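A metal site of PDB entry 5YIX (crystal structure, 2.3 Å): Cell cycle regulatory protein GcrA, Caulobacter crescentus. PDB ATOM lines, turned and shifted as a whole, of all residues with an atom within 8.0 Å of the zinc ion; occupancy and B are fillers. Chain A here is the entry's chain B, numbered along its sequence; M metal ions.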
ATOM      1  N   MET A  34      21.183 -22.641  23.447  1.00  0.00           N
ATOM      2  CA  MET A  34      22.545 -22.388  23.910  1.00  0.00           C
ATOM      3  C   MET A  34      23.208 -23.702  24.272  1.00  0.00           C
ATOM      4  O   MET A  34      22.537 -24.642  24.700  1.00  0.00           O
ATOM      5  CB  MET A  34      22.550 -21.439  25.102  1.00  0.00           C
ATOM      6  CG  MET A  34      22.192 -20.015  24.747  1.00  0.00           C
ATOM      7  SD  MET A  34      21.965 -19.001  26.212  1.00  0.00           S
ATOM      8  CE  MET A  34      23.588 -19.083  26.964  1.00  0.00           C
ATOM      9  N   CYS A  35      24.520 -23.779  24.107  1.00  0.00           N
ATOM     10  CA  CYS A  35      25.248 -25.031  24.288  1.00  0.00           C
ATOM     11  C   CYS A  35      25.331 -25.407  25.766  1.00  0.00           C
ATOM     12  O   CYS A  35      25.835 -24.631  26.591  1.00  0.00           O
ATOM     13  CB  CYS A  35      26.647 -24.950  23.685  1.00  0.00           C
ATOM     14  SG  CYS A  35      27.599 -26.483  23.851  1.00  0.00           S
ATOM     15  N   LYS A  36      24.858 -26.613  26.078  1.00  0.00           N
ATOM     16  CA  LYS A  36      24.773 -27.080  27.466  1.00  0.00           C
ATOM     17  C   LYS A  36      26.038 -27.791  27.951  1.00  0.00           C
ATOM     18  O   LYS A  36      26.020 -28.438  28.998  1.00  0.00           O
ATOM     19  CB  LYS A  36      23.582 -28.026  27.639  1.00  0.00           C
ATOM     20  CG  LYS A  36      22.210 -27.453  27.305  1.00  0.00           C
ATOM     21  CD  LYS A  36      21.138 -28.554  27.412  1.00  0.00           C
ATOM     22  CE  LYS A  36      19.735 -28.009  27.150  1.00  0.00           C
ATOM     23  NZ  LYS A  36      19.523 -26.714  27.890  1.00  0.00           N
ATOM     24  N   TRP A  37      27.120 -27.688  27.172  1.00  0.00           N
ATOM     25  CA  TRP A  37      28.384 -28.334  27.508  1.00  0.00           C
ATOM     26  C   TRP A  37      28.913 -27.785  28.821  1.00  0.00           C
ATOM     27  O   TRP A  37      29.166 -26.593  28.949  1.00  0.00           O
ATOM     28  CB  TRP A  37      29.426 -28.144  26.398  1.00  0.00           C
ATOM     29  CG  TRP A  37      30.675 -28.932  26.648  1.00  0.00           C
ATOM     30  CD1 TRP A  37      31.859 -28.461  27.119  1.00  0.00           C
ATOM     31  CD2 TRP A  37      30.854 -30.346  26.461  1.00  0.00           C
ATOM     32  NE1 TRP A  37      32.759 -29.481  27.231  1.00  0.00           N
ATOM     33  CE2 TRP A  37      32.167 -30.654  26.836  1.00  0.00           C
ATOM     34  CE3 TRP A  37      30.021 -31.380  26.019  1.00  0.00           C
ATOM     35  CZ2 TRP A  37      32.689 -31.950  26.779  1.00  0.00           C
ATOM     36  CZ3 TRP A  37      30.530 -32.665  25.966  1.00  0.00           C
ATOM     37  CH2 TRP A  37      31.857 -32.943  26.353  1.00  0.00           C
ATOM     38  N   PRO A  38      29.061 -28.661  29.819  1.00  0.00           N
ATOM     39  CA  PRO A  38      29.523 -28.177  31.115  1.00  0.00           C
ATOM     40  C   PRO A  38      31.048 -28.038  31.171  1.00  0.00           C
ATOM     41  O   PRO A  38      31.765 -28.911  30.680  1.00  0.00           O
ATOM     42  CB  PRO A  38      29.014 -29.240  32.088  1.00  0.00           C
ATOM     43  CG  PRO A  38      28.906 -30.491  31.272  1.00  0.00           C
ATOM     44  CD  PRO A  38      28.724 -30.096  29.824  1.00  0.00           C
ATOM     45  N   ILE A  39      31.527 -26.938  31.743  1.00  0.00           N
ATOM     46  CA  ILE A  39      32.957 -26.677  31.883  1.00  0.00           C
ATOM     47  C   ILE A  39      33.342 -26.586  33.368  1.00  0.00           C
ATOM     48  O   ILE A  39      32.789 -25.771  34.111  1.00  0.00           O
ATOM     49  CB  ILE A  39      33.373 -25.377  31.167  1.00  0.00           C
ATOM     50  CG1 ILE A  39      33.029 -25.462  29.677  1.00  0.00           C
ATOM     51  CG2 ILE A  39      34.864 -25.081  31.359  1.00  0.00           C
ATOM     52  CD1 ILE A  39      32.993 -24.123  28.996  1.00  0.00           C
ATOM     53  N   PHE A  49      28.668 -23.197  31.582  1.00  0.00           N
ATOM     54  CA  PHE A  49      28.347 -23.957  30.385  1.00  0.00           C
ATOM     55  C   PHE A  49      28.890 -23.206  29.177  1.00  0.00           C
ATOM     56  O   PHE A  49      29.018 -21.978  29.235  1.00  0.00           O
ATOM     57  CB  PHE A  49      26.838 -24.180  30.235  1.00  0.00           C
ATOM     58  CG  PHE A  49      26.203 -24.951  31.359  1.00  0.00           C
ATOM     59  CD1 PHE A  49      26.166 -26.335  31.340  1.00  0.00           C
ATOM     60  CD2 PHE A  49      25.632 -24.284  32.438  1.00  0.00           C
ATOM     61  CE1 PHE A  49      25.578 -27.043  32.367  1.00  0.00           C
ATOM     62  CE2 PHE A  49      25.042 -24.993  33.487  1.00  0.00           C
ATOM     63  CZ  PHE A  49      25.024 -26.368  33.457  1.00  0.00           C
ATOM     64  N   CYS A  50      29.205 -23.923  28.107  1.00  0.00           N
ATOM     65  CA  CYS A  50      29.701 -23.323  26.857  1.00  0.00           C
ATOM     66  C   CYS A  50      28.823 -22.130  26.431  1.00  0.00           C
ATOM     67  O   CYS A  50      29.272 -20.972  26.388  1.00  0.00           O
ATOM     68  CB  CYS A  50      29.774 -24.392  25.763  1.00  0.00           C
ATOM     69  SG  CYS A  50      30.096 -23.838  24.038  1.00  0.00           S
ATOM     70  N   GLY A  51      27.565 -22.408  26.119  1.00  0.00           N
ATOM     71  CA  GLY A  51      26.590 -21.345  25.931  1.00  0.00           C
ATOM     72  C   GLY A  51      26.622 -20.683  24.572  1.00  0.00           C
ATOM     73  O   GLY A  51      25.941 -19.680  24.340  1.00  0.00           O
ATOM     74  N   ARG A  52      27.422 -21.234  23.660  1.00  0.00           N
ATOM     75  CA  ARG A  52      27.432 -20.760  22.289  1.00  0.00           C
ATOM     76  C   ARG A  52      26.222 -21.347  21.577  1.00  0.00           C
ATOM     77  O   ARG A  52      25.471 -22.123  22.175  1.00  0.00           O
ATOM     78  CB  ARG A  52      28.739 -21.139  21.614  1.00  0.00           C
ATOM     79  CG  ARG A  52      29.963 -20.562  22.299  1.00  0.00           C
ATOM     80  CD  ARG A  52      31.181 -20.512  21.380  1.00  0.00           C
ATOM     81  NE  ARG A  52      31.582 -21.841  20.908  1.00  0.00           N
ATOM     82  CZ  ARG A  52      32.584 -22.541  21.441  1.00  0.00           C
ATOM     83  NH1 ARG A  52      32.889 -23.748  20.954  1.00  0.00           N
ATOM     84  NH2 ARG A  52      33.274 -22.048  22.454  1.00  0.00           N
ATOM     85  N   ARG A  53      26.004 -20.957  20.324  1.00  0.00           N
ATOM     86  CA  ARG A  53      24.784 -21.350  19.626  1.00  0.00           C
ATOM     87  C   ARG A  53      24.726 -22.861  19.438  1.00  0.00           C
ATOM     88  O   ARG A  53      25.632 -23.485  18.885  1.00  0.00           O
ATOM     89  CB  ARG A  53      24.659 -20.631  18.281  1.00  0.00           C
ATOM     90  CG  ARG A  53      23.502 -21.109  17.399  1.00  0.00           C
ATOM     91  CD  ARG A  53      22.161 -21.022  18.106  1.00  0.00           C
ATOM     92  NE  ARG A  53      21.066 -21.581  17.314  1.00  0.00           N
ATOM     93  CZ  ARG A  53      19.931 -20.942  17.038  1.00  0.00           C
ATOM     94  NH1 ARG A  53      19.736 -19.701  17.484  1.00  0.00           N
ATOM     95  NH2 ARG A  53      18.988 -21.523  16.315  1.00  0.00           N
ATOM     96  N   SER A  54      23.656 -23.445  19.940  1.00  0.00           N
ATOM     97  CA  SER A  54      23.420 -24.867  19.815  1.00  0.00           C
ATOM     98  C   SER A  54      22.822 -25.168  18.460  1.00  0.00           C
ATOM     99  O   SER A  54      22.135 -24.330  17.868  1.00  0.00           O
ATOM    100  CB  SER A  54      22.500 -25.346  20.927  1.00  0.00           C
ATOM    101  OG  SER A  54      22.123 -26.695  20.723  1.00  0.00           O
ATOM    102  N   PRO A  58      21.596 -30.404  22.366  1.00  0.00           N
ATOM    103  CA  PRO A  58      22.004 -29.541  23.490  1.00  0.00           C
ATOM    104  C   PRO A  58      23.319 -28.804  23.230  1.00  0.00           C
ATOM    105  O   PRO A  58      23.700 -27.906  24.003  1.00  0.00           O
ATOM    106  CB  PRO A  58      22.153 -30.536  24.639  1.00  0.00           C
ATOM    107  CG  PRO A  58      22.512 -31.835  23.981  1.00  0.00           C
ATOM    108  CD  PRO A  58      21.799 -31.836  22.642  1.00  0.00           C
ATOM    109  N   TYR A  59      24.009 -29.158  22.159  1.00  0.00           N
ATOM    110  CA  TYR A  59      25.403 -28.736  21.982  1.00  0.00           C
ATOM    111  C   TYR A  59      25.715 -28.058  20.654  1.00  0.00           C
ATOM    112  O   TYR A  59      25.138 -28.398  19.617  1.00  0.00           O
ATOM    113  CB  TYR A  59      26.340 -29.947  22.128  1.00  0.00           C
ATOM    114  CG  TYR A  59      26.223 -30.716  23.429  1.00  0.00           C
ATOM    115  CD1 TYR A  59      26.217 -30.073  24.663  1.00  0.00           C
ATOM    116  CD2 TYR A  59      26.135 -32.107  23.416  1.00  0.00           C
ATOM    117  CE1 TYR A  59      26.131 -30.794  25.839  1.00  0.00           C
ATOM    118  CE2 TYR A  59      26.040 -32.825  24.578  1.00  0.00           C
ATOM    119  CZ  TYR A  59      26.045 -32.173  25.777  1.00  0.00           C
ATOM    120  OH  TYR A  59      25.957 -32.911  26.916  1.00  0.00           O
ATOM    121  N   CYS A  60      26.656 -27.122  20.672  1.00  0.00           N
ATOM    122  CA  CYS A  60      27.299 -26.648  19.458  1.00  0.00           C
ATOM    123  C   CYS A  60      27.955 -27.828  18.757  1.00  0.00           C
ATOM    124  O   CYS A  60      28.125 -28.893  19.355  1.00  0.00           O
ATOM    125  CB  CYS A  60      28.341 -25.578  19.756  1.00  0.00           C
ATOM    126  SG  CYS A  60      29.778 -26.219  20.693  1.00  0.00           S
ATOM    127  N   VAL A  61      28.342 -27.630  17.495  1.00  0.00           N
ATOM    128  CA  VAL A  61      28.970 -28.688  16.704  1.00  0.00           C
ATOM    129  C   VAL A  61      30.226 -29.289  17.383  1.00  0.00           C
ATOM    130  O   VAL A  61      30.381 -30.503  17.447  1.00  0.00           O
ATOM    131  CB  VAL A  61      29.364 -28.168  15.294  1.00  0.00           C
ATOM    132  CG1 VAL A  61      30.179 -26.860  15.394  1.00  0.00           C
ATOM    133  CG2 VAL A  61      30.117 -29.237  14.508  1.00  0.00           C
ATOM    134  N   GLU A  62      31.087 -28.426  17.904  1.00  0.00           N
ATOM    135  CA  GLU A  62      32.328 -28.886  18.530  1.00  0.00           C
ATOM    136  C   GLU A  62      32.056 -29.848  19.711  1.00  0.00           C
ATOM    137  O   GLU A  62      32.620 -30.962  19.793  1.00  0.00           O
ATOM    138  CB  GLU A  62      33.130 -27.673  19.011  1.00  0.00           C
ATOM    139  CG  GLU A  62      34.556 -27.994  19.412  1.00  0.00           C
ATOM    140  CD  GLU A  62      35.323 -26.780  19.931  1.00  0.00           C
ATOM    141  OE1 GLU A  62      36.475 -26.570  19.504  1.00  0.00           O
ATOM    142  OE2 GLU A  62      34.798 -26.050  20.792  1.00  0.00           O
ATOM    143  N   HIS A  63      31.165 -29.434  20.600  1.00  0.00           N
ATOM    144  CA  HIS A  63      30.879 -30.230  21.784  1.00  0.00           C
ATOM    145  C   HIS A  63      29.981 -31.402  21.478  1.00  0.00           C
ATOM    146  O   HIS A  63      30.039 -32.408  22.174  1.00  0.00           O
ATOM    147  CB  HIS A  63      30.269 -29.329  22.855  1.00  0.00           C
ATOM    148  CG  HIS A  63      31.277 -28.420  23.470  1.00  0.00           C
ATOM    149  ND1 HIS A  63      31.027 -27.097  23.751  1.00  0.00           N
ATOM    150  CD2 HIS A  63      32.574 -28.648  23.830  1.00  0.00           C
ATOM    151  CE1 HIS A  63      32.107 -26.550  24.280  1.00  0.00           C
ATOM    152  NE2 HIS A  63      33.062 -27.465  24.335  1.00  0.00           N
ATOM    153  N   ALA A  64      29.181 -31.299  20.421  1.00  0.00           N
ATOM    154  CA  ALA A  64      28.441 -32.462  19.930  1.00  0.00           C
ATOM    155  C   ALA A  64      29.420 -33.527  19.480  1.00  0.00           C
ATOM    156  O   ALA A  64      29.224 -34.714  19.756  1.00  0.00           O
ATOM    157  CB  ALA A  64      27.507 -32.082  18.796  1.00  0.00           C
HETATM  158 ZN    ZN M   1      29.645 -25.756  22.985  1.00  0.00          ZN
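The zinc ion is bound by a ring nitrogen (ND1) of His 63, the side-chain sulfur of Cys 50, the side-chain sulfur of Cys 35 and the side-chain sulfur of Cys 60.
Of the 19 residues printed, 4 come within 4 Å of the zinc ion. Along chain A the residues within 4 Å of the zinc ion span positions 35 to 63.
The backbone NH (N) of Cys 50 sits at hydrogen-bond distance from the backbone carbonyl oxygen (O) of Trp 37 (2.8 Å). SG of Cys 50 sits close to N of Arg 52 (3.8 Å). The side-chain sulfur (SG) of Cys 35 sits close to the backbone NH (N) of Trp 37 (3.6 Å). O of Arg 52 sits at hydrogen-bond distance from N of Cys 35 (2.7 Å). The backbone carbonyl oxygen of Cys 35 sits at hydrogen-bond distance from the backbone NH of Gly 51, at 2.9 Å. The side-chain sulfur (SG) of Cys 60 lies close to the backbone NH (N) of Glu 62 (3.8 Å).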
